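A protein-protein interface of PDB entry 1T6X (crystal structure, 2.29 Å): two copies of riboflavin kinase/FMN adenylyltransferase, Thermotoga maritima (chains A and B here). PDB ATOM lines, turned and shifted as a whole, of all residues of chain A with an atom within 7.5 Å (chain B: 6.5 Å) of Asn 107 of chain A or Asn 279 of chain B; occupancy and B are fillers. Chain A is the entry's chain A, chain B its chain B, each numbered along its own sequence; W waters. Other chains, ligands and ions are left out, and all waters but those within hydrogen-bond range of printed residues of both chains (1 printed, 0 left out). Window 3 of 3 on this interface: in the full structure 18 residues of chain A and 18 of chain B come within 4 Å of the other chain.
Of the 12 printed residues of chain A, 4 touch a printed residue of chain B. Hydrophobic or aromatic side chains of chain A within 4 Å of the printed part of chain B: Ala 108. Among the printed residues, no Asp or Glu carboxylate lies within 4 Å of a Lys or Arg side-chain nitrogen of the other chain.
The side-chain amide nitrogen of Asn 107 of chain A sits close to the side-chain amide nitrogen of Asn 279 of chain B (3.2 Å). The backbone NH (N) of Asn 107 of chain A is in hydrogen-bond range of the side-chain carboxylate (OD1) of Asp 282 of chain B (2.8 Å).
Arg 103 of chain A touches Arg 278 of chain B (CZ to NH2, 3.3 Å). CE of Lys 106 of chain A touches OD2 of Asp 282 of chain B (2.9 Å). Asn 107 of chain A touches Arg 278 of chain B. CB of Ala 108 of chain A touches NH1 of Arg 278 of chain B, at 3.5 Å.
O of Leu 80 of chain A lies within hydrogen-bond range of N of Lys 106 of chain A (2.6 Å). The guanidinium group (NH1) of Arg 103 of chain A is in hydrogen-bond range of the backbone carbonyl oxygen (O) of Ala 108 of chain A (2.6 Å). The side-chain hydroxyl of Ser 109 of chain A is in hydrogen-bond range of the backbone carbonyl oxygen of Lys 106 of chain A (2.9 Å).
Water W1 lies within hydrogen-bond range of the side-chain amide oxygen (OD1) of Asn 279 of chain B (2.6 Å) and the side-chain amide nitrogen (ND2) of Asn 107 of chain A (3.3 Å).
No position is printed for both chains. Of the 6 pairs that touch across the chains among the printed residues, none has its exchanged pair printed and touching as well.
Of chain B, only Arg 278 (3.5 Å), Asn 279 (3.2 Å) and Asp 282 (2.8 Å) come within 4 Å of Asn 107 of chain A. Asn 279 of chain B touches just one residue of chain A: Asn 107. Printed residues of chain B within 4 Å of Arg 103 of chain A: Arg 278. Of the printed residues of chain A, Arg 278 of chain B touches Arg 103 (3.3 Å), Asn 107 (3.5 Å) and Ala 108 (3.5 Å). The nearest residue of chain A that does not touch Asn 279 of chain B is Lys 106 of chain A (6.1 Å).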
ATOM      1  N   LYS A  78      -9.048 -28.645 -15.342  1.00  0.00           N
ATOM      2  CA  LYS A  78      -8.029 -28.019 -16.178  1.00  0.00           C
ATOM      3  C   LYS A  78      -7.656 -28.820 -17.427  1.00  0.00           C
ATOM      4  O   LYS A  78      -7.349 -28.247 -18.469  1.00  0.00           O
ATOM      5  CB  LYS A  78      -6.770 -27.732 -15.339  1.00  0.00           C
ATOM      6  CG  LYS A  78      -5.938 -28.992 -15.002  1.00  0.00           C
ATOM      7  CD  LYS A  78      -4.920 -28.750 -13.899  1.00  0.00           C
ATOM      8  CE  LYS A  78      -4.083 -30.015 -13.629  1.00  0.00           C
ATOM      9  NZ  LYS A  78      -3.193 -30.380 -14.786  1.00  0.00           N
ATOM     10  N   ASP A  79      -7.687 -30.143 -17.347  1.00  0.00           N
ATOM     11  CA  ASP A  79      -7.299 -30.929 -18.511  1.00  0.00           C
ATOM     12  C   ASP A  79      -8.386 -31.372 -19.475  1.00  0.00           C
ATOM     13  O   ASP A  79      -8.083 -31.995 -20.490  1.00  0.00           O
ATOM     14  CB  ASP A  79      -6.488 -32.142 -18.067  1.00  0.00           C
ATOM     15  CG  ASP A  79      -5.233 -31.741 -17.327  1.00  0.00           C
ATOM     16  OD1 ASP A  79      -4.474 -30.896 -17.863  1.00  0.00           O
ATOM     17  OD2 ASP A  79      -5.008 -32.262 -16.214  1.00  0.00           O
ATOM     18  N   LEU A  80      -9.638 -31.044 -19.178  1.00  0.00           N
ATOM     19  CA  LEU A  80     -10.745 -31.433 -20.051  1.00  0.00           C
ATOM     20  C   LEU A  80     -10.847 -30.615 -21.316  1.00  0.00           C
ATOM     21  O   LEU A  80     -10.454 -29.463 -21.365  1.00  0.00           O
ATOM     22  CB  LEU A  80     -12.084 -31.291 -19.340  1.00  0.00           C
ATOM     23  CG  LEU A  80     -12.251 -31.987 -18.014  1.00  0.00           C
ATOM     24  CD1 LEU A  80     -13.546 -31.504 -17.334  1.00  0.00           C
ATOM     25  CD2 LEU A  80     -12.254 -33.465 -18.249  1.00  0.00           C
ATOM     26  N   PRO A  82     -13.289 -28.828 -24.203  1.00  0.00           N
ATOM     27  CA  PRO A  82     -14.547 -28.089 -24.055  1.00  0.00           C
ATOM     28  C   PRO A  82     -15.668 -29.106 -24.033  1.00  0.00           C
ATOM     29  O   PRO A  82     -16.546 -29.072 -23.173  1.00  0.00           O
ATOM     30  CB  PRO A  82     -14.577 -27.227 -25.306  1.00  0.00           C
ATOM     31  CG  PRO A  82     -13.141 -26.924 -25.532  1.00  0.00           C
ATOM     32  CD  PRO A  82     -12.450 -28.243 -25.267  1.00  0.00           C
ATOM     33  N   ARG A 103     -13.689 -18.446 -20.130  1.00  0.00           N
ATOM     34  CA  ARG A 103     -12.927 -19.484 -20.808  1.00  0.00           C
ATOM     35  C   ARG A 103     -12.915 -20.801 -20.004  1.00  0.00           C
ATOM     36  O   ARG A 103     -13.047 -20.792 -18.791  1.00  0.00           O
ATOM     37  CB  ARG A 103     -11.505 -18.968 -21.029  1.00  0.00           C
ATOM     38  CG  ARG A 103     -11.442 -17.881 -22.073  1.00  0.00           C
ATOM     39  CD  ARG A 103     -11.115 -18.521 -23.379  1.00  0.00           C
ATOM     40  NE  ARG A 103     -11.575 -17.760 -24.517  1.00  0.00           N
ATOM     41  CZ  ARG A 103     -11.356 -18.129 -25.772  1.00  0.00           C
ATOM     42  NH1 ARG A 103     -10.688 -19.248 -26.034  1.00  0.00           N
ATOM     43  NH2 ARG A 103     -11.792 -17.377 -26.766  1.00  0.00           N
ATOM     44  N   PHE A 104     -12.764 -21.937 -20.674  1.00  0.00           N
ATOM     45  CA  PHE A 104     -12.740 -23.216 -19.959  1.00  0.00           C
ATOM     46  C   PHE A 104     -12.105 -24.311 -20.806  1.00  0.00           C
ATOM     47  O   PHE A 104     -11.986 -24.181 -22.027  1.00  0.00           O
ATOM     48  CB  PHE A 104     -14.166 -23.626 -19.538  1.00  0.00           C
ATOM     49  CG  PHE A 104     -15.079 -23.961 -20.693  1.00  0.00           C
ATOM     50  CD1 PHE A 104     -15.157 -25.267 -21.188  1.00  0.00           C
ATOM     51  CD2 PHE A 104     -15.874 -22.980 -21.284  1.00  0.00           C
ATOM     52  CE1 PHE A 104     -16.026 -25.583 -22.262  1.00  0.00           C
ATOM     53  CE2 PHE A 104     -16.733 -23.280 -22.346  1.00  0.00           C
ATOM     54  CZ  PHE A 104     -16.806 -24.588 -22.833  1.00  0.00           C
ATOM     55  N   GLY A 105     -11.680 -25.382 -20.145  1.00  0.00           N
ATOM     56  CA  GLY A 105     -11.060 -26.478 -20.857  1.00  0.00           C
ATOM     57  C   GLY A 105      -9.592 -26.268 -21.176  1.00  0.00           C
ATOM     58  O   GLY A 105      -9.071 -25.153 -21.107  1.00  0.00           O
ATOM     59  N   LYS A 106      -8.930 -27.356 -21.546  1.00  0.00           N
ATOM     60  CA  LYS A 106      -7.526 -27.316 -21.894  1.00  0.00           C
ATOM     61  C   LYS A 106      -7.249 -26.129 -22.810  1.00  0.00           C
ATOM     62  O   LYS A 106      -7.981 -25.888 -23.771  1.00  0.00           O
ATOM     63  CB  LYS A 106      -7.134 -28.611 -22.605  1.00  0.00           C
ATOM     64  CG  LYS A 106      -5.638 -28.860 -22.674  1.00  0.00           C
ATOM     65  CD  LYS A 106      -5.050 -29.030 -21.274  1.00  0.00           C
ATOM     66  CE  LYS A 106      -3.563 -29.368 -21.321  1.00  0.00           C
ATOM     67  NZ  LYS A 106      -3.324 -30.659 -22.011  1.00  0.00           N
ATOM     68  N   ASN A 107      -6.181 -25.400 -22.500  1.00  0.00           N
ATOM     69  CA  ASN A 107      -5.759 -24.240 -23.273  1.00  0.00           C
ATOM     70  C   ASN A 107      -6.834 -23.178 -23.395  1.00  0.00           C
ATOM     71  O   ASN A 107      -6.879 -22.494 -24.409  1.00  0.00           O
ATOM     72  CB  ASN A 107      -5.336 -24.665 -24.672  1.00  0.00           C
ATOM     73  CG  ASN A 107      -4.214 -25.678 -24.657  1.00  0.00           C
ATOM     74  OD1 ASN A 107      -3.257 -25.569 -23.878  1.00  0.00           O
ATOM     75  ND2 ASN A 107      -4.314 -26.665 -25.526  1.00  0.00           N
ATOM     76  N   ALA A 108      -7.688 -23.036 -22.380  1.00  0.00           N
ATOM     77  CA  ALA A 108      -8.779 -22.053 -22.419  1.00  0.00           C
ATOM     78  C   ALA A 108      -9.401 -22.049 -23.826  1.00  0.00           C
ATOM     79  O   ALA A 108      -9.750 -21.004 -24.375  1.00  0.00           O
ATOM     80  CB  ALA A 108      -8.245 -20.674 -22.073  1.00  0.00           C
ATOM     81  N   SER A 109      -9.528 -23.242 -24.399  1.00  0.00           N
ATOM     82  CA  SER A 109     -10.065 -23.403 -25.744  1.00  0.00           C
ATOM     83  C   SER A 109     -11.576 -23.289 -25.820  1.00  0.00           C
ATOM     84  O   SER A 109     -12.115 -23.078 -26.893  1.00  0.00           O
ATOM     85  CB  SER A 109      -9.645 -24.758 -26.313  1.00  0.00           C
ATOM     86  OG  SER A 109     -10.273 -25.803 -25.595  1.00  0.00           O
ATOM     87  N   GLY A 110     -12.257 -23.445 -24.694  1.00  0.00           N
ATOM     88  CA  GLY A 110     -13.706 -23.340 -24.704  1.00  0.00           C
ATOM     89  C   GLY A 110     -14.192 -21.944 -24.338  1.00  0.00           C
ATOM     90  O   GLY A 110     -13.685 -21.323 -23.398  1.00  0.00           O
ATOM     91  N   VAL B 274      -2.095 -16.591 -31.308  1.00  0.00           N
ATOM     92  CA  VAL B 274      -2.907 -16.557 -30.103  1.00  0.00           C
ATOM     93  C   VAL B 274      -3.068 -17.996 -29.619  1.00  0.00           C
ATOM     94  O   VAL B 274      -2.970 -18.283 -28.425  1.00  0.00           O
ATOM     95  CB  VAL B 274      -4.295 -15.915 -30.351  1.00  0.00           C
ATOM     96  CG1 VAL B 274      -4.124 -14.568 -31.039  1.00  0.00           C
ATOM     97  CG2 VAL B 274      -5.176 -16.851 -31.166  1.00  0.00           C
ATOM     98  N   LYS B 275      -3.278 -18.906 -30.556  1.00  0.00           N
ATOM     99  CA  LYS B 275      -3.428 -20.309 -30.201  1.00  0.00           C
ATOM    100  C   LYS B 275      -2.158 -20.772 -29.490  1.00  0.00           C
ATOM    101  O   LYS B 275      -2.198 -21.228 -28.347  1.00  0.00           O
ATOM    102  CB  LYS B 275      -3.638 -21.169 -31.452  1.00  0.00           C
ATOM    103  CG  LYS B 275      -3.701 -22.671 -31.169  1.00  0.00           C
ATOM    104  CD  LYS B 275      -3.208 -23.505 -32.354  1.00  0.00           C
ATOM    105  CE  LYS B 275      -4.022 -23.250 -33.620  1.00  0.00           C
ATOM    106  NZ  LYS B 275      -3.477 -23.974 -34.811  1.00  0.00           N
ATOM    107  N   SER B 276      -1.031 -20.648 -30.181  1.00  0.00           N
ATOM    108  CA  SER B 276       0.240 -21.073 -29.620  1.00  0.00           C
ATOM    109  C   SER B 276       0.451 -20.471 -28.226  1.00  0.00           C
ATOM    110  O   SER B 276       0.945 -21.145 -27.316  1.00  0.00           O
ATOM    111  CB  SER B 276       1.384 -20.692 -30.555  1.00  0.00           C
ATOM    112  OG  SER B 276       2.523 -21.468 -30.235  1.00  0.00           O
ATOM    113  N   ALA B 277       0.031 -19.221 -28.054  1.00  0.00           N
ATOM    114  CA  ALA B 277       0.171 -18.569 -26.769  1.00  0.00           C
ATOM    115  C   ALA B 277      -0.634 -19.341 -25.731  1.00  0.00           C
ATOM    116  O   ALA B 277      -0.106 -19.712 -24.671  1.00  0.00           O
ATOM    117  CB  ALA B 277      -0.303 -17.133 -26.851  1.00  0.00           C
ATOM    118  N   ARG B 278      -1.910 -19.591 -26.036  1.00  0.00           N
ATOM    119  CA  ARG B 278      -2.776 -20.333 -25.115  1.00  0.00           C
ATOM    120  C   ARG B 278      -2.189 -21.682 -24.754  1.00  0.00           C
ATOM    121  O   ARG B 278      -2.329 -22.141 -23.636  1.00  0.00           O
ATOM    122  CB  ARG B 278      -4.179 -20.510 -25.699  1.00  0.00           C
ATOM    123  CG  ARG B 278      -4.999 -19.228 -25.706  1.00  0.00           C
ATOM    124  CD  ARG B 278      -6.422 -19.491 -26.168  1.00  0.00           C
ATOM    125  NE  ARG B 278      -7.206 -18.274 -26.337  1.00  0.00           N
ATOM    126  CZ  ARG B 278      -7.708 -17.537 -25.345  1.00  0.00           C
ATOM    127  NH1 ARG B 278      -7.513 -17.871 -24.075  1.00  0.00           N
ATOM    128  NH2 ARG B 278      -8.450 -16.470 -25.629  1.00  0.00           N
ATOM    129  N   ASN B 279      -1.511 -22.326 -25.682  1.00  0.00           N
ATOM    130  CA  ASN B 279      -0.919 -23.614 -25.332  1.00  0.00           C
ATOM    131  C   ASN B 279       0.243 -23.424 -24.341  1.00  0.00           C
ATOM    132  O   ASN B 279       0.311 -24.106 -23.302  1.00  0.00           O
ATOM    133  CB  ASN B 279      -0.443 -24.348 -26.585  1.00  0.00           C
ATOM    134  CG  ASN B 279      -1.149 -25.670 -26.773  1.00  0.00           C
ATOM    135  OD1 ASN B 279      -0.837 -26.667 -26.102  1.00  0.00           O
ATOM    136  ND2 ASN B 279      -2.128 -25.686 -27.676  1.00  0.00           N
ATOM    137  N   MET B 280       1.139 -22.487 -24.654  1.00  0.00           N
ATOM    138  CA  MET B 280       2.272 -22.220 -23.786  1.00  0.00           C
ATOM    139  C   MET B 280       1.749 -21.811 -22.416  1.00  0.00           C
ATOM    140  O   MET B 280       2.272 -22.237 -21.368  1.00  0.00           O
ATOM    141  CB  MET B 280       3.150 -21.119 -24.387  1.00  0.00           C
ATOM    142  CG  MET B 280       3.819 -21.545 -25.690  1.00  0.00           C
ATOM    143  SD  MET B 280       4.664 -20.246 -26.598  1.00  0.00           S
ATOM    144  CE  MET B 280       6.326 -20.434 -25.886  1.00  0.00           C
ATOM    145  N   ILE B 281       0.690 -21.007 -22.425  1.00  0.00           N
ATOM    146  CA  ILE B 281       0.106 -20.553 -21.186  1.00  0.00           C
ATOM    147  C   ILE B 281      -0.358 -21.754 -20.393  1.00  0.00           C
ATOM    148  O   ILE B 281      -0.127 -21.835 -19.192  1.00  0.00           O
ATOM    149  CB  ILE B 281      -1.054 -19.602 -21.441  1.00  0.00           C
ATOM    150  CG1 ILE B 281      -0.507 -18.311 -22.063  1.00  0.00           C
ATOM    151  CG2 ILE B 281      -1.792 -19.344 -20.156  1.00  0.00           C
ATOM    152  CD1 ILE B 281      -1.538 -17.230 -22.351  1.00  0.00           C
ATOM    153  N   ASP B 282      -0.987 -22.711 -21.060  1.00  0.00           N
ATOM    154  CA  ASP B 282      -1.445 -23.899 -20.357  1.00  0.00           C
ATOM    155  C   ASP B 282      -0.219 -24.655 -19.788  1.00  0.00           C
ATOM    156  O   ASP B 282      -0.228 -25.100 -18.633  1.00  0.00           O
ATOM    157  CB  ASP B 282      -2.251 -24.789 -21.310  1.00  0.00           C
ATOM    158  CG  ASP B 282      -3.213 -25.718 -20.577  1.00  0.00           C
ATOM    159  OD1 ASP B 282      -4.392 -25.339 -20.386  1.00  0.00           O
ATOM    160  OD2 ASP B 282      -2.774 -26.826 -20.181  1.00  0.00           O
ATOM    161  N   ASP B 283       0.840 -24.771 -20.589  1.00  0.00           N
ATOM    162  CA  ASP B 283       2.070 -25.464 -20.166  1.00  0.00           C
ATOM    163  C   ASP B 283       2.655 -24.823 -18.913  1.00  0.00           C
ATOM    164  O   ASP B 283       3.043 -25.516 -17.955  1.00  0.00           O
ATOM    165  CB  ASP B 283       3.135 -25.425 -21.267  1.00  0.00           C
ATOM    166  CG  ASP B 283       2.678 -26.070 -22.561  1.00  0.00           C
ATOM    167  OD1 ASP B 283       1.956 -27.089 -22.524  1.00  0.00           O
ATOM    168  OD2 ASP B 283       3.063 -25.560 -23.633  1.00  0.00           O
ATOM    169  N   ILE B 284       2.723 -23.492 -18.926  1.00  0.00           N
ATOM    170  CA  ILE B 284       3.259 -22.764 -17.791  1.00  0.00           C
ATOM    171  C   ILE B 284       2.455 -23.118 -16.543  1.00  0.00           C
ATOM    172  O   ILE B 284       3.018 -23.460 -15.503  1.00  0.00           O
ATOM    173  CB  ILE B 284       3.203 -21.247 -18.025  1.00  0.00           C
ATOM    174  CG1 ILE B 284       4.091 -20.869 -19.200  1.00  0.00           C
ATOM    175  CG2 ILE B 284       3.679 -20.515 -16.788  1.00  0.00           C
ATOM    176  CD1 ILE B 284       4.028 -19.394 -19.563  1.00  0.00           C
HETATM  177  O   HOH W   1      -1.965 -28.913 -25.654  1.00  0.00           O
